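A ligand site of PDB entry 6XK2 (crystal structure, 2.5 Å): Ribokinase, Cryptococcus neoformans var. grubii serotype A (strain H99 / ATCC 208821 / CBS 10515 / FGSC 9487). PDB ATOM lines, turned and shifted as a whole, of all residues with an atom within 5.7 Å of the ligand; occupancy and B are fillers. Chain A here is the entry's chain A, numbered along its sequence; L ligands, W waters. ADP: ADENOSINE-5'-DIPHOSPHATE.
The side-chain sulfur (SG) of Cys 308 sits close to the backbone NH (N) of Phe 283, 3.7 Å away.
The side-chain amide oxygen (OD1) of Asn 195 is in hydrogen-bond range of the backbone NH (N) of Glu 198.
The side-chain sulfur (SG) of Cys 308 sits at hydrogen-bond distance from the backbone carbonyl oxygen (O) of Cys 304.
The backbone carbonyl oxygen (O) of Ala 279 lies within hydrogen-bond range of the side-chain sulfur (SG) of Cys 308.
O1B of the ligand is in hydrogen-bond range of ND2 of Asn 195, 3.4 Å away.
The backbone NH (N) of Gly 248 is in hydrogen-bond range of an oxygen (O2A) of the ligand, at 2.8 Å.
O of Gly 251 sits at hydrogen-bond distance from O3' of the ligand (3.2 Å).
The side-chain hydroxyl of Thr 246 lies within hydrogen-bond range of an oxygen (O2A) of the ligand (3.0 Å).
Water W1 lies within hydrogen-bond range of O3B of the ligand (2.5 Å) and OG1 of Thr 246 (2.8 Å).
Water W2 lies within hydrogen-bond range of an oxygen (O2') of the ligand (2.6 Å), the backbone NH (N) of Ala 267 (2.8 Å) and the backbone carbonyl oxygen (O) of Leu 305 (2.8 Å).
Water W3 bridges OE1 of Glu 198 (2.7 Å) and O3B of the ligand (3.3 Å).
Leu 247 touches the ligand (N to O2A, 3.7 Å).
Ala 249 touches the ligand (CB to N6, 3.5 Å).
Ile 252 touches the ligand.
CB of Ala 266 touches N3 of the ligand (3.9 Å).
Ala 279 touches the ligand (CB to O4', 3.4 Å).
Gly 280 touches the ligand.
Leu 305 touches the ligand.
CB of Cys 308 touches O4' of the ligand, 3.5 Å away.
Hydrophobic or aromatic side chains within 4 Å of the ligand: Ala 249, Ile 252, Ala 266, Ala 279 and Leu 305.
The nearest printed residue that does not touch the ligand is Thr 276 (4.02 Å).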
ATOM      1  N   LYS A  51       1.374   3.740  24.849  1.00  0.00           N
ATOM      2  CA  LYS A  51       2.353   3.389  25.872  1.00  0.00           C
ATOM      3  C   LYS A  51       1.745   2.510  26.951  1.00  0.00           C
ATOM      4  O   LYS A  51       2.370   1.538  27.399  1.00  0.00           O
ATOM      5  CB  LYS A  51       2.927   4.651  26.521  1.00  0.00           C
ATOM      6  CG  LYS A  51       3.809   5.451  25.598  1.00  0.00           C
ATOM      7  CD  LYS A  51       5.256   5.239  25.942  1.00  0.00           C
ATOM      8  CE  LYS A  51       6.096   5.337  24.700  1.00  0.00           C
ATOM      9  NZ  LYS A  51       7.515   5.197  25.107  1.00  0.00           N
ATOM     10  N   ASN A 195      15.042   7.320  28.125  1.00  0.00           N
ATOM     11  CA  ASN A 195      16.153   7.209  27.200  1.00  0.00           C
ATOM     12  C   ASN A 195      17.071   8.406  27.411  1.00  0.00           C
ATOM     13  O   ASN A 195      16.807   9.261  28.264  1.00  0.00           O
ATOM     14  CB  ASN A 195      15.666   7.086  25.740  1.00  0.00           C
ATOM     15  CG  ASN A 195      14.747   8.226  25.317  1.00  0.00           C
ATOM     16  OD1 ASN A 195      15.054   9.400  25.499  1.00  0.00           O
ATOM     17  ND2 ASN A 195      13.607   7.866  24.723  1.00  0.00           N
ATOM     18  N   GLU A 196      18.165   8.485  26.642  1.00  0.00           N
ATOM     19  CA  GLU A 196      19.122   9.549  26.901  1.00  0.00           C
ATOM     20  C   GLU A 196      18.530  10.929  26.614  1.00  0.00           C
ATOM     21  O   GLU A 196      18.848  11.886  27.324  1.00  0.00           O
ATOM     22  CB  GLU A 196      20.430   9.328  26.111  1.00  0.00           C
ATOM     23  CG  GLU A 196      20.347   9.485  24.594  1.00  0.00           C
ATOM     24  CD  GLU A 196      20.046   8.174  23.874  1.00  0.00           C
ATOM     25  OE1 GLU A 196      19.372   7.297  24.471  1.00  0.00           O
ATOM     26  OE2 GLU A 196      20.483   8.018  22.715  1.00  0.00           O
ATOM     27  N   GLU A 198      15.365  11.858  27.022  1.00  0.00           N
ATOM     28  CA  GLU A 198      14.471  12.214  28.120  1.00  0.00           C
ATOM     29  C   GLU A 198      15.272  12.555  29.376  1.00  0.00           C
ATOM     30  O   GLU A 198      14.903  13.479  30.125  1.00  0.00           O
ATOM     31  CB  GLU A 198      13.514  11.060  28.361  1.00  0.00           C
ATOM     32  CG  GLU A 198      12.447  10.987  27.284  1.00  0.00           C
ATOM     33  CD  GLU A 198      11.808   9.618  27.172  1.00  0.00           C
ATOM     34  OE1 GLU A 198      12.351   8.641  27.747  1.00  0.00           O
ATOM     35  OE2 GLU A 198      10.757   9.531  26.492  1.00  0.00           O
ATOM     36  N   THR A 246      17.819   3.777  28.936  1.00  0.00           N
ATOM     37  CA  THR A 246      18.032   2.918  27.773  1.00  0.00           C
ATOM     38  C   THR A 246      18.751   3.681  26.673  1.00  0.00           C
ATOM     39  O   THR A 246      18.508   4.876  26.452  1.00  0.00           O
ATOM     40  CB  THR A 246      16.691   2.395  27.256  1.00  0.00           C
ATOM     41  OG1 THR A 246      15.930   3.498  26.777  1.00  0.00           O
ATOM     42  CG2 THR A 246      15.918   1.670  28.343  1.00  0.00           C
ATOM     43  N   LEU A 247      19.638   2.993  25.958  1.00  0.00           N
ATOM     44  CA  LEU A 247      20.488   3.632  24.960  1.00  0.00           C
ATOM     45  C   LEU A 247      20.366   2.961  23.598  1.00  0.00           C
ATOM     46  O   LEU A 247      21.341   2.903  22.856  1.00  0.00           O
ATOM     47  CB  LEU A 247      21.946   3.653  25.411  1.00  0.00           C
ATOM     48  CG  LEU A 247      22.188   4.188  26.826  1.00  0.00           C
ATOM     49  CD1 LEU A 247      23.636   3.980  27.190  1.00  0.00           C
ATOM     50  CD2 LEU A 247      21.805   5.646  26.869  1.00  0.00           C
ATOM     51  N   GLY A 248      19.190   2.433  23.274  1.00  0.00           N
ATOM     52  CA  GLY A 248      19.022   1.803  21.980  1.00  0.00           C
ATOM     53  C   GLY A 248      20.018   0.674  21.768  1.00  0.00           C
ATOM     54  O   GLY A 248      20.243  -0.173  22.638  1.00  0.00           O
ATOM     55  N   ALA A 249      20.661   0.692  20.611  1.00  0.00           N
ATOM     56  CA  ALA A 249      21.552  -0.407  20.240  1.00  0.00           C
ATOM     57  C   ALA A 249      22.762  -0.505  21.160  1.00  0.00           C
ATOM     58  O   ALA A 249      23.447  -1.546  21.138  1.00  0.00           O
ATOM     59  CB  ALA A 249      22.021  -0.230  18.797  1.00  0.00           C
ATOM     60  N   GLY A 251      22.676  -0.442  24.468  1.00  0.00           N
ATOM     61  CA  GLY A 251      22.357  -1.130  25.714  1.00  0.00           C
ATOM     62  C   GLY A 251      21.613  -0.269  26.708  1.00  0.00           C
ATOM     63  O   GLY A 251      20.813   0.575  26.320  1.00  0.00           O
ATOM     64  N   ILE A 252      21.866  -0.487  28.010  1.00  0.00           N
ATOM     65  CA  ILE A 252      21.154   0.218  29.075  1.00  0.00           C
ATOM     66  C   ILE A 252      22.131   0.651  30.145  1.00  0.00           C
ATOM     67  O   ILE A 252      23.242   0.107  30.276  1.00  0.00           O
ATOM     68  CB  ILE A 252      20.047  -0.638  29.717  1.00  0.00           C
ATOM     69  CG1 ILE A 252      20.660  -1.862  30.395  1.00  0.00           C
ATOM     70  CG2 ILE A 252      19.032  -1.074  28.691  1.00  0.00           C
ATOM     71  CD1 ILE A 252      19.780  -2.457  31.419  1.00  0.00           C
ATOM     72  N   ALA A 266      23.344  -4.310  24.802  1.00  0.00           N
ATOM     73  CA  ALA A 266      22.204  -4.937  24.146  1.00  0.00           C
ATOM     74  C   ALA A 266      22.525  -6.391  23.823  1.00  0.00           C
ATOM     75  O   ALA A 266      23.682  -6.780  23.625  1.00  0.00           O
ATOM     76  CB  ALA A 266      21.849  -4.194  22.854  1.00  0.00           C
ATOM     77  N   ALA A 267      21.479  -7.215  23.788  1.00  0.00           N
ATOM     78  CA  ALA A 267      21.669  -8.612  23.465  1.00  0.00           C
ATOM     79  C   ALA A 267      22.129  -8.733  22.025  1.00  0.00           C
ATOM     80  O   ALA A 267      21.652  -8.017  21.140  1.00  0.00           O
ATOM     81  CB  ALA A 267      20.365  -9.372  23.669  1.00  0.00           C
ATOM     82  N   LEU A 269      21.975 -10.034  18.459  1.00  0.00           N
ATOM     83  CA  LEU A 269      20.812 -10.501  17.720  1.00  0.00           C
ATOM     84  C   LEU A 269      21.100 -11.834  17.027  1.00  0.00           C
ATOM     85  O   LEU A 269      22.231 -12.112  16.632  1.00  0.00           O
ATOM     86  CB  LEU A 269      20.370  -9.469  16.685  1.00  0.00           C
ATOM     87  CG  LEU A 269      19.996  -8.096  17.226  1.00  0.00           C
ATOM     88  CD1 LEU A 269      19.658  -7.148  16.065  1.00  0.00           C
ATOM     89  CD2 LEU A 269      18.840  -8.192  18.215  1.00  0.00           C
ATOM     90  N   VAL A 273      17.718  -6.936  12.116  1.00  0.00           N
ATOM     91  CA  VAL A 273      16.752  -5.982  12.645  1.00  0.00           C
ATOM     92  C   VAL A 273      15.566  -5.876  11.681  1.00  0.00           C
ATOM     93  O   VAL A 273      15.724  -5.568  10.502  1.00  0.00           O
ATOM     94  CB  VAL A 273      17.387  -4.603  12.847  1.00  0.00           C
ATOM     95  CG1 VAL A 273      16.351  -3.611  13.334  1.00  0.00           C
ATOM     96  CG2 VAL A 273      18.529  -4.684  13.830  1.00  0.00           C
ATOM     97  N   THR A 276      12.475  -1.565  15.244  1.00  0.00           N
ATOM     98  CA  THR A 276      12.796  -1.241  16.634  1.00  0.00           C
ATOM     99  C   THR A 276      11.650  -0.548  17.364  1.00  0.00           C
ATOM    100  O   THR A 276      11.823  -0.167  18.533  1.00  0.00           O
ATOM    101  CB  THR A 276      14.034  -0.334  16.726  1.00  0.00           C
ATOM    102  OG1 THR A 276      13.744   0.940  16.122  1.00  0.00           O
ATOM    103  CG2 THR A 276      15.236  -0.971  16.035  1.00  0.00           C
ATOM    104  N   ALA A 279      10.472  -1.209  21.324  1.00  0.00           N
ATOM    105  CA  ALA A 279      11.515  -1.809  22.156  1.00  0.00           C
ATOM    106  C   ALA A 279      11.549  -1.181  23.540  1.00  0.00           C
ATOM    107  O   ALA A 279      11.711  -1.888  24.535  1.00  0.00           O
ATOM    108  CB  ALA A 279      12.879  -1.684  21.474  1.00  0.00           C
ATOM    109  N   GLY A 280      11.375   0.141  23.630  1.00  0.00           N
ATOM    110  CA  GLY A 280      11.333   0.788  24.936  1.00  0.00           C
ATOM    111  C   GLY A 280      10.162   0.316  25.768  1.00  0.00           C
ATOM    112  O   GLY A 280      10.314  -0.001  26.959  1.00  0.00           O
ATOM    113  N   ASP A 281       8.985   0.205  25.150  1.00  0.00           N
ATOM    114  CA  ASP A 281       7.825  -0.298  25.865  1.00  0.00           C
ATOM    115  C   ASP A 281       7.982  -1.781  26.225  1.00  0.00           C
ATOM    116  O   ASP A 281       7.628  -2.186  27.340  1.00  0.00           O
ATOM    117  CB  ASP A 281       6.555  -0.071  25.061  1.00  0.00           C
ATOM    118  CG  ASP A 281       6.289   1.394  24.832  1.00  0.00           C
ATOM    119  OD1 ASP A 281       5.655   1.754  23.817  1.00  0.00           O
ATOM    120  OD2 ASP A 281       6.712   2.187  25.712  1.00  0.00           O
ATOM    121  N   PHE A 283      10.736  -3.084  26.961  1.00  0.00           N
ATOM    122  CA  PHE A 283      11.647  -3.061  28.105  1.00  0.00           C
ATOM    123  C   PHE A 283      10.913  -2.703  29.395  1.00  0.00           C
ATOM    124  O   PHE A 283      11.054  -3.385  30.408  1.00  0.00           O
ATOM    125  CB  PHE A 283      12.796  -2.070  27.856  1.00  0.00           C
ATOM    126  CG  PHE A 283      13.781  -2.022  28.981  1.00  0.00           C
ATOM    127  CD1 PHE A 283      13.550  -1.214  30.072  1.00  0.00           C
ATOM    128  CD2 PHE A 283      14.893  -2.828  28.989  1.00  0.00           C
ATOM    129  CE1 PHE A 283      14.424  -1.186  31.127  1.00  0.00           C
ATOM    130  CE2 PHE A 283      15.789  -2.801  30.042  1.00  0.00           C
ATOM    131  CZ  PHE A 283      15.552  -1.987  31.112  1.00  0.00           C
ATOM    132  N   CYS A 304      15.203  -8.492  30.450  1.00  0.00           N
ATOM    133  CA  CYS A 304      14.737  -7.380  29.617  1.00  0.00           C
ATOM    134  C   CYS A 304      15.515  -7.287  28.319  1.00  0.00           C
ATOM    135  O   CYS A 304      14.927  -7.080  27.242  1.00  0.00           O
ATOM    136  CB  CYS A 304      14.870  -6.062  30.367  1.00  0.00           C
ATOM    137  SG  CYS A 304      13.691  -5.764  31.644  1.00  0.00           S
ATOM    138  N   LEU A 305      16.842  -7.398  28.403  1.00  0.00           N
ATOM    139  CA  LEU A 305      17.663  -7.225  27.211  1.00  0.00           C
ATOM    140  C   LEU A 305      17.407  -8.342  26.207  1.00  0.00           C
ATOM    141  O   LEU A 305      17.285  -8.068  25.000  1.00  0.00           O
ATOM    142  CB  LEU A 305      19.140  -7.167  27.605  1.00  0.00           C
ATOM    143  CG  LEU A 305      19.479  -5.926  28.434  1.00  0.00           C
ATOM    144  CD1 LEU A 305      20.868  -6.032  29.071  1.00  0.00           C
ATOM    145  CD2 LEU A 305      19.359  -4.647  27.606  1.00  0.00           C
ATOM    146  N   CYS A 308      14.143  -7.734  24.552  1.00  0.00           N
ATOM    147  CA  CYS A 308      14.201  -6.653  23.569  1.00  0.00           C
ATOM    148  C   CYS A 308      14.968  -7.046  22.312  1.00  0.00           C
ATOM    149  O   CYS A 308      14.639  -6.572  21.221  1.00  0.00           O
ATOM    150  CB  CYS A 308      14.828  -5.410  24.207  1.00  0.00           C
ATOM    151  SG  CYS A 308      13.791  -4.636  25.456  1.00  0.00           S
ATOM    152  N   GLY A 309      15.972  -7.916  22.448  1.00  0.00           N
ATOM    153  CA  GLY A 309      16.636  -8.422  21.265  1.00  0.00           C
ATOM    154  C   GLY A 309      15.656  -9.143  20.359  1.00  0.00           C
ATOM    155  O   GLY A 309      15.620  -8.904  19.152  1.00  0.00           O
ATOM    156  N   VAL A 312      13.187  -6.538  18.462  1.00  0.00           N
ATOM    157  CA  VAL A 312      13.604  -5.780  17.281  1.00  0.00           C
ATOM    158  C   VAL A 312      13.823  -6.667  16.060  1.00  0.00           C
ATOM    159  O   VAL A 312      13.989  -6.155  14.942  1.00  0.00           O
ATOM    160  CB  VAL A 312      14.882  -4.965  17.576  1.00  0.00           C
ATOM    161  CG1 VAL A 312      14.609  -3.921  18.645  1.00  0.00           C
ATOM    162  CG2 VAL A 312      16.014  -5.888  17.964  1.00  0.00           C
HETATM  163  PB  ADP L   1      13.184   3.811  23.482  1.00  0.00           P
HETATM  164  O1B ADP L   1      14.190   4.936  23.162  1.00  0.00           O
HETATM  165  O2B ADP L   1      12.211   3.580  22.272  1.00  0.00           O
HETATM  166  O3B ADP L   1      12.442   4.053  24.780  1.00  0.00           O
HETATM  167  PA  ADP L   1      15.472   2.030  23.022  1.00  0.00           P
HETATM  168  O1A ADP L   1      15.690   2.549  21.646  1.00  0.00           O
HETATM  169  O2A ADP L   1      16.538   2.578  24.008  1.00  0.00           O
HETATM  170  O3A ADP L   1      14.026   2.453  23.538  1.00  0.00           O
HETATM  171  O5' ADP L   1      15.336   0.435  23.123  1.00  0.00           O
HETATM  172  C5' ADP L   1      15.268  -0.282  24.378  1.00  0.00           C
HETATM  173  C4' ADP L   1      16.137  -1.505  24.300  1.00  0.00           C
HETATM  174  O4' ADP L   1      15.859  -2.249  23.100  1.00  0.00           O
HETATM  175  C3' ADP L   1      17.635  -1.228  24.245  1.00  0.00           C
HETATM  176  O3' ADP L   1      18.160  -0.980  25.532  1.00  0.00           O
HETATM  177  C2' ADP L   1      18.159  -2.522  23.612  1.00  0.00           C
HETATM  178  O2' ADP L   1      18.298  -3.549  24.585  1.00  0.00           O
HETATM  179  C1' ADP L   1      17.046  -2.827  22.593  1.00  0.00           C
HETATM  180  N9  ADP L   1      17.317  -2.262  21.278  1.00  0.00           N
HETATM  181  C8  ADP L   1      16.840  -1.084  20.770  1.00  0.00           C
HETATM  182  N7  ADP L   1      17.330  -0.788  19.582  1.00  0.00           N
HETATM  183  C5  ADP L   1      18.163  -1.839  19.298  1.00  0.00           C
HETATM  184  C6  ADP L   1      18.989  -2.130  18.185  1.00  0.00           C
HETATM  185  N6  ADP L   1      19.096  -1.326  17.118  1.00  0.00           N
HETATM  186  N1  ADP L   1      19.689  -3.282  18.199  1.00  0.00           N
HETATM  187  C2  ADP L   1      19.582  -4.087  19.255  1.00  0.00           C
HETATM  188  N3  ADP L   1      18.850  -3.917  20.371  1.00  0.00           N
HETATM  189  C4  ADP L   1      18.166  -2.782  20.328  1.00  0.00           C
HETATM  190  O   HOH W   1      13.232   4.126  27.201  1.00  0.00           O
HETATM  191  O   HOH W   2      18.969  -6.006  24.002  1.00  0.00           O
HETATM  192  O   HOH W   3      11.575   6.148  27.231  1.00  0.00           O
